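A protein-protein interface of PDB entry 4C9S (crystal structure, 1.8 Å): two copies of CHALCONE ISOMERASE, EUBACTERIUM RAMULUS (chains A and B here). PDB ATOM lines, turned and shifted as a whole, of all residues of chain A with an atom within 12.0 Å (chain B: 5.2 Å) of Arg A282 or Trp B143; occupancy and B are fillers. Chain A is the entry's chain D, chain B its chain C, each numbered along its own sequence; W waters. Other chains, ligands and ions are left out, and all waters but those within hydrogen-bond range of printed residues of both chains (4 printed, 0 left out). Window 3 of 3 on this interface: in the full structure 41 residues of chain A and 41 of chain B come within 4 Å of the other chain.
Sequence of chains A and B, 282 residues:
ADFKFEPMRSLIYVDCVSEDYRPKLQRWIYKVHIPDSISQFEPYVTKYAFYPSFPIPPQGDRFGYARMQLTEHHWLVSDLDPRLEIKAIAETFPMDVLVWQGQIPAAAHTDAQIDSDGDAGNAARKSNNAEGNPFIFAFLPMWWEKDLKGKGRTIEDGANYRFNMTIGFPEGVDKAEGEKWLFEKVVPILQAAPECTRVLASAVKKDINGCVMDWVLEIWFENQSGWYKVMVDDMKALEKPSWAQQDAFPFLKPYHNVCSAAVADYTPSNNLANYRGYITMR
NE1 of Trp B144 lies within hydrogen-bond range of OXT of Arg A282, at 2.8 Å. O of Arg A282 is in salt-bridge range of NH2 of Arg B9. O of Met B142 is in hydrogen-bond range of NH1 of Arg A282 (2.8 Å). The indole nitrogen of Trp B143 sits close to the guanidinium group of Arg A282. A ring nitrogen (NE2) of His B74 sits at hydrogen-bond distance from the guanidinium group (NH1) of Arg A282 (3.0 Å). The chain-end carboxylate (O) of Arg A282 is in salt-bridge range of the guanidinium group (NH2) of Arg B162 (2.9 Å). The guanidinium group (NH1) of Arg B162 sits at hydrogen-bond distance from the backbone carbonyl oxygen (O) of Met A281 (3.0 Å).
The guanidinium group (NH2) of Arg B162 is in salt-bridge range of the side-chain carboxylate (OE2) of Glu B218, 2.9 Å away. NH2 of Arg B9 is in salt-bridge range of OE2 of Glu B72.
Among the printed residues, pairs that only touch across the chains: Met A281 with Arg B9 (3.7 Å) and Met A281 with Glu B218 (3.9 Å).
Tyr A278 touches none of the printed residues of chain B. Ile A279 touches none of the printed residues of chain B. Of the printed residues of chain B, Met A281 touches Arg B9, Arg B162 and Glu B218. Arg A282 touches just these residues of chain B: Arg B9, His B74, Met B142, Trp B143, Trp B144 and Arg B162. No residue of chain A comes within 4 Å of Pro B7. Of chain A, only Met A281 (3.7 Å) and Arg A282 (3.9 Å) come within 4 Å of Arg B9. Printed residues of chain A within 4 Å of His B74: Arg A282. No residue of chain A comes within 4 Å of Pro B141. Trp B143 touches one residue of chain A. Trp B144 touches just one residue of chain A: Arg A282. Printed residues of chain A within 4 Å of Arg B162: Met A281 and Arg A282. Printed residues of chain A within 4 Å of Glu B218: Met A281. The nearest printed residue of chain A that does not touch His B74 is Met A281 (7.2 Å).
Along chain A the printed residues that touch a printed residue of chain B span positions 281 to 282. Hydrophobic or aromatic side chains of chain B within 4 Å of the printed part of chain A: His B74, Trp B143 and Trp B144. Along chain B the printed residues that touch a printed residue of chain A span positions 9 to 218. Among the printed residues, 9 pairs touch across the chains. Among the printed residues, no Asp or Glu carboxylate lies within 4 Å of a Lys or Arg side-chain nitrogen of the other chain.
No position is printed for both chains. Of the 9 pairs that touch across the chains among the printed residues, none has its exchanged pair printed and touching as well.
Water W3 lies within hydrogen-bond range of the side-chain carboxylate of Glu B218 (2.6 Å), the chain-end carboxylate of Arg A282 (2.6 Å) and the guanidinium group of Arg B9 (2.8 Å). Water W4 lies within hydrogen-bond range of the side-chain carboxylate (OE2) of Glu B72 (2.7 Å) and the backbone NH (N) of Arg A282 (2.8 Å). Water W1 lies within hydrogen-bond range of the backbone carbonyl oxygen of Met B142 and the chain-end carboxylate of Arg A282. Water W2 bridges the guanidinium group (NH2) of Arg A282 (3.0 Å) and the indole nitrogen (NE1) of Trp B143 (3.4 Å).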
ATOM      1  N   TYR A 278      -5.214  34.546 -33.217  1.00  0.00           N
ATOM      2  CA  TYR A 278      -6.006  33.806 -32.200  1.00  0.00           C
ATOM      3  C   TYR A 278      -5.032  33.165 -31.208  1.00  0.00           C
ATOM      4  O   TYR A 278      -4.662  32.006 -31.319  1.00  0.00           O
ATOM      5  CB  TYR A 278      -6.908  32.767 -32.873  1.00  0.00           C
ATOM      6  CG  TYR A 278      -7.964  32.143 -31.990  1.00  0.00           C
ATOM      7  CD1 TYR A 278      -9.130  32.848 -31.686  1.00  0.00           C
ATOM      8  CD2 TYR A 278      -7.849  30.833 -31.518  1.00  0.00           C
ATOM      9  CE1 TYR A 278     -10.149  32.295 -30.928  1.00  0.00           C
ATOM     10  CE2 TYR A 278      -8.838  30.265 -30.711  1.00  0.00           C
ATOM     11  CZ  TYR A 278      -9.980  30.976 -30.422  1.00  0.00           C
ATOM     12  OH  TYR A 278     -11.002  30.438 -29.671  1.00  0.00           O
ATOM     13  N   ILE A 279      -4.598  33.953 -30.257  1.00  0.00           N
ATOM     14  CA  ILE A 279      -3.636  33.523 -29.268  1.00  0.00           C
ATOM     15  C   ILE A 279      -4.443  32.775 -28.180  1.00  0.00           C
ATOM     16  O   ILE A 279      -5.421  33.314 -27.665  1.00  0.00           O
ATOM     17  CB  ILE A 279      -2.927  34.757 -28.670  1.00  0.00           C
ATOM     18  CG1 ILE A 279      -2.167  35.568 -29.759  1.00  0.00           C
ATOM     19  CG2 ILE A 279      -1.989  34.384 -27.543  1.00  0.00           C
ATOM     20  CD1 ILE A 279      -1.383  34.714 -30.752  1.00  0.00           C
ATOM     21  N   THR A 280      -3.996  31.598 -27.800  1.00  0.00           N
ATOM     22  CA  THR A 280      -4.737  30.784 -26.850  1.00  0.00           C
ATOM     23  C   THR A 280      -4.135  30.833 -25.440  1.00  0.00           C
ATOM     24  O   THR A 280      -2.922  30.938 -25.281  1.00  0.00           O
ATOM     25  CB  THR A 280      -4.838  29.336 -27.330  1.00  0.00           C
ATOM     26  OG1 THR A 280      -3.535  28.792 -27.556  1.00  0.00           O
ATOM     27  CG2 THR A 280      -5.607  29.253 -28.629  1.00  0.00           C
ATOM     28  N   MET A 281      -5.020  30.785 -24.441  1.00  0.00           N
ATOM     29  CA  MET A 281      -4.644  30.733 -23.053  1.00  0.00           C
ATOM     30  C   MET A 281      -3.755  29.505 -22.763  1.00  0.00           C
ATOM     31  O   MET A 281      -4.002  28.404 -23.257  1.00  0.00           O
ATOM     32  CB  MET A 281      -5.893  30.718 -22.141  1.00  0.00           C
ATOM     33  CG  MET A 281      -5.511  30.913 -20.664  1.00  0.00           C
ATOM     34  SD  MET A 281      -6.968  31.055 -19.579  1.00  0.00           S
ATOM     35  CE  MET A 281      -7.860  29.771 -20.085  1.00  0.00           C
ATOM     36  N   ARG A 282      -2.752  29.729 -21.931  1.00  0.00           N
ATOM     37  CA  ARG A 282      -1.772  28.711 -21.483  1.00  0.00           C
ATOM     38  C   ARG A 282      -2.370  27.863 -20.313  1.00  0.00           C
ATOM     39  O   ARG A 282      -3.586  27.900 -20.046  1.00  0.00           O
ATOM     40  CB  ARG A 282      -0.473  29.428 -21.067  1.00  0.00           C
ATOM     41  CG  ARG A 282       0.180  30.248 -22.212  1.00  0.00           C
ATOM     42  CD  ARG A 282       1.429  31.075 -21.802  1.00  0.00           C
ATOM     43  NE  ARG A 282       2.460  30.143 -21.496  1.00  0.00           N
ATOM     44  CZ  ARG A 282       2.765  29.651 -20.300  1.00  0.00           C
ATOM     45  NH1 ARG A 282       2.336  30.189 -19.182  1.00  0.00           N
ATOM     46  NH2 ARG A 282       3.623  28.650 -20.248  1.00  0.00           N
ATOM     47  OXT ARG A 282      -1.630  27.145 -19.596  1.00  0.00           O
ATOM     48  N   PRO B   7      10.042  33.596 -12.223  1.00  0.00           N
ATOM     49  CA  PRO B   7       8.979  33.567 -13.221  1.00  0.00           C
ATOM     50  C   PRO B   7       7.745  32.855 -12.694  1.00  0.00           C
ATOM     51  O   PRO B   7       7.862  31.726 -12.154  1.00  0.00           O
ATOM     52  CB  PRO B   7       9.613  32.801 -14.374  1.00  0.00           C
ATOM     53  CG  PRO B   7      10.687  31.970 -13.770  1.00  0.00           C
ATOM     54  CD  PRO B   7      11.216  32.786 -12.653  1.00  0.00           C
ATOM     55  N   ARG B   9       3.098  32.583 -13.026  1.00  0.00           N
ATOM     56  CA  ARG B   9       1.833  32.956 -13.521  1.00  0.00           C
ATOM     57  C   ARG B   9       0.891  33.088 -12.301  1.00  0.00           C
ATOM     58  O   ARG B   9       0.869  32.187 -11.478  1.00  0.00           O
ATOM     59  CB  ARG B   9       1.298  31.856 -14.412  1.00  0.00           C
ATOM     60  CG  ARG B   9      -0.053  32.146 -15.045  1.00  0.00           C
ATOM     61  CD  ARG B   9      -0.547  30.906 -15.758  1.00  0.00           C
ATOM     62  NE  ARG B   9      -1.754  31.175 -16.544  1.00  0.00           N
ATOM     63  CZ  ARG B   9      -2.773  30.341 -16.679  1.00  0.00           C
ATOM     64  NH1 ARG B   9      -2.763  29.113 -16.106  1.00  0.00           N
ATOM     65  NH2 ARG B   9      -3.802  30.728 -17.415  1.00  0.00           N
ATOM     66  N   GLU B  72      -5.008  37.536 -15.160  1.00  0.00           N
ATOM     67  CA  GLU B  72      -3.822  36.705 -15.278  1.00  0.00           C
ATOM     68  C   GLU B  72      -2.601  37.609 -15.470  1.00  0.00           C
ATOM     69  O   GLU B  72      -2.593  38.477 -16.365  1.00  0.00           O
ATOM     70  CB  GLU B  72      -3.974  35.801 -16.481  1.00  0.00           C
ATOM     71  CG  GLU B  72      -2.847  34.823 -16.721  1.00  0.00           C
ATOM     72  CD  GLU B  72      -2.787  34.371 -18.166  1.00  0.00           C
ATOM     73  OE1 GLU B  72      -2.750  35.183 -19.119  1.00  0.00           O
ATOM     74  OE2 GLU B  72      -2.779  33.142 -18.386  1.00  0.00           O
ATOM     75  N   HIS B  74       1.805  37.321 -15.801  1.00  0.00           N
ATOM     76  CA  HIS B  74       3.016  36.573 -15.820  1.00  0.00           C
ATOM     77  C   HIS B  74       4.147  37.515 -15.380  1.00  0.00           C
ATOM     78  O   HIS B  74       4.418  38.557 -16.029  1.00  0.00           O
ATOM     79  CB  HIS B  74       3.267  36.052 -17.224  1.00  0.00           C
ATOM     80  CG  HIS B  74       2.414  34.906 -17.652  1.00  0.00           C
ATOM     81  ND1 HIS B  74       1.149  35.043 -18.101  1.00  0.00           N
ATOM     82  CD2 HIS B  74       2.729  33.543 -17.827  1.00  0.00           C
ATOM     83  CE1 HIS B  74       0.667  33.816 -18.422  1.00  0.00           C
ATOM     84  NE2 HIS B  74       1.637  32.929 -18.280  1.00  0.00           N
ATOM     85  N   PRO B 141       3.694  28.247 -10.832  1.00  0.00           N
ATOM     86  CA  PRO B 141       4.744  28.270 -11.867  1.00  0.00           C
ATOM     87  C   PRO B 141       4.108  28.601 -13.245  1.00  0.00           C
ATOM     88  O   PRO B 141       2.883  28.467 -13.429  1.00  0.00           O
ATOM     89  CB  PRO B 141       5.328  26.830 -11.818  1.00  0.00           C
ATOM     90  CG  PRO B 141       4.215  26.034 -11.243  1.00  0.00           C
ATOM     91  CD  PRO B 141       3.364  26.887 -10.373  1.00  0.00           C
ATOM     92  N   MET B 142       4.908  29.064 -14.212  1.00  0.00           N
ATOM     93  CA  MET B 142       4.352  29.416 -15.510  1.00  0.00           C
ATOM     94  C   MET B 142       3.866  28.177 -16.300  1.00  0.00           C
ATOM     95  O   MET B 142       3.091  28.314 -17.238  1.00  0.00           O
ATOM     96  CB  MET B 142       5.394  30.175 -16.344  1.00  0.00           C
ATOM     97  CG  MET B 142       5.726  31.569 -15.840  1.00  0.00           C
ATOM     98  SD  MET B 142       6.617  32.431 -17.174  1.00  0.00           S
ATOM     99  CE  MET B 142       6.629  34.065 -16.466  1.00  0.00           C
ATOM    100  N   TRP B 143       4.345  26.979 -15.907  1.00  0.00           N
ATOM    101  CA  TRP B 143       3.981  25.736 -16.584  1.00  0.00           C
ATOM    102  C   TRP B 143       3.223  24.837 -15.630  1.00  0.00           C
ATOM    103  O   TRP B 143       3.623  24.644 -14.466  1.00  0.00           O
ATOM    104  CB  TRP B 143       5.192  25.050 -17.180  1.00  0.00           C
ATOM    105  CG  TRP B 143       5.941  25.986 -18.074  1.00  0.00           C
ATOM    106  CD1 TRP B 143       5.749  26.185 -19.423  1.00  0.00           C
ATOM    107  CD2 TRP B 143       6.941  26.971 -17.674  1.00  0.00           C
ATOM    108  NE1 TRP B 143       6.549  27.200 -19.896  1.00  0.00           N
ATOM    109  CE2 TRP B 143       7.317  27.693 -18.873  1.00  0.00           C
ATOM    110  CE3 TRP B 143       7.605  27.263 -16.487  1.00  0.00           C
ATOM    111  CZ2 TRP B 143       8.281  28.694 -18.849  1.00  0.00           C
ATOM    112  CZ3 TRP B 143       8.546  28.272 -16.483  1.00  0.00           C
ATOM    113  CH2 TRP B 143       8.883  28.963 -17.622  1.00  0.00           C
ATOM    114  N   TRP B 144       2.134  24.275 -16.128  1.00  0.00           N
ATOM    115  CA  TRP B 144       1.356  23.333 -15.329  1.00  0.00           C
ATOM    116  C   TRP B 144       2.279  22.223 -14.841  1.00  0.00           C
ATOM    117  O   TRP B 144       3.073  21.648 -15.614  1.00  0.00           O
ATOM    118  CB  TRP B 144       0.235  22.705 -16.138  1.00  0.00           C
ATOM    119  CG  TRP B 144      -0.828  23.690 -16.506  1.00  0.00           C
ATOM    120  CD1 TRP B 144      -0.994  24.332 -17.715  1.00  0.00           C
ATOM    121  CD2 TRP B 144      -1.854  24.207 -15.623  1.00  0.00           C
ATOM    122  NE1 TRP B 144      -2.058  25.186 -17.683  1.00  0.00           N
ATOM    123  CE2 TRP B 144      -2.652  25.130 -16.422  1.00  0.00           C
ATOM    124  CE3 TRP B 144      -2.238  23.925 -14.326  1.00  0.00           C
ATOM    125  CZ2 TRP B 144      -3.760  25.738 -15.923  1.00  0.00           C
ATOM    126  CZ3 TRP B 144      -3.331  24.561 -13.814  1.00  0.00           C
ATOM    127  CH2 TRP B 144      -4.099  25.458 -14.595  1.00  0.00           C
ATOM    128  N   GLU B 145       2.111  21.858 -13.581  1.00  0.00           N
ATOM    129  CA  GLU B 145       2.925  20.769 -13.005  1.00  0.00           C
ATOM    130  C   GLU B 145       2.472  19.366 -13.365  1.00  0.00           C
ATOM    131  O   GLU B 145       3.293  18.456 -13.477  1.00  0.00           O
ATOM    132  CB  GLU B 145       2.961  20.946 -11.492  1.00  0.00           C
ATOM    133  CG  GLU B 145       3.652  22.245 -11.146  1.00  0.00           C
ATOM    134  CD  GLU B 145       3.759  22.520  -9.666  1.00  0.00           C
ATOM    135  OE1 GLU B 145       2.822  22.173  -8.934  1.00  0.00           O
ATOM    136  OE2 GLU B 145       4.787  23.135  -9.278  1.00  0.00           O
ATOM    137  N   ARG B 162     -13.275  26.037 -20.726  1.00  0.00           N
ATOM    138  CA  ARG B 162     -12.171  25.788 -19.828  1.00  0.00           C
ATOM    139  C   ARG B 162     -12.550  26.177 -18.424  1.00  0.00           C
ATOM    140  O   ARG B 162     -12.701  27.365 -18.107  1.00  0.00           O
ATOM    141  CB  ARG B 162     -10.948  26.570 -20.304  1.00  0.00           C
ATOM    142  CG  ARG B 162     -10.588  26.186 -21.710  1.00  0.00           C
ATOM    143  CD  ARG B 162      -9.473  26.974 -22.387  1.00  0.00           C
ATOM    144  NE  ARG B 162      -8.232  26.880 -21.696  1.00  0.00           N
ATOM    145  CZ  ARG B 162      -7.012  27.099 -22.219  1.00  0.00           C
ATOM    146  NH1 ARG B 162      -6.800  27.369 -23.503  1.00  0.00           N
ATOM    147  NH2 ARG B 162      -5.987  27.056 -21.394  1.00  0.00           N
ATOM    148  N   SER B 202      -1.685  22.436 -10.893  1.00  0.00           N
ATOM    149  CA  SER B 202      -0.487  22.908 -10.238  1.00  0.00           C
ATOM    150  C   SER B 202      -0.775  23.173  -8.774  1.00  0.00           C
ATOM    151  O   SER B 202      -1.861  23.577  -8.415  1.00  0.00           O
ATOM    152  CB  SER B 202       0.068  24.196 -10.900  1.00  0.00           C
ATOM    153  OG  SER B 202       0.638  23.905 -12.171  1.00  0.00           O
ATOM    154  N   GLU B 218      -7.350  23.020 -14.068  1.00  0.00           N
ATOM    155  CA  GLU B 218      -8.146  23.430 -15.179  1.00  0.00           C
ATOM    156  C   GLU B 218      -8.694  22.184 -15.840  1.00  0.00           C
ATOM    157  O   GLU B 218      -7.946  21.230 -16.064  1.00  0.00           O
ATOM    158  CB  GLU B 218      -7.364  24.326 -16.113  1.00  0.00           C
ATOM    159  CG  GLU B 218      -8.302  25.103 -17.041  1.00  0.00           C
ATOM    160  CD  GLU B 218      -7.563  26.196 -17.804  1.00  0.00           C
ATOM    161  OE1 GLU B 218      -7.254  27.227 -17.157  1.00  0.00           O
ATOM    162  OE2 GLU B 218      -7.365  26.011 -19.010  1.00  0.00           O
HETATM  163  O   HOH W   1       0.287  27.820 -17.542  1.00  0.00           O
HETATM  164  O   HOH W   2       4.393  26.993 -22.579  1.00  0.00           O
HETATM  165  O   HOH W   3      -4.948  28.255 -17.810  1.00  0.00           O
HETATM  166  O   HOH W   4      -2.113  32.280 -20.907  1.00  0.00           O
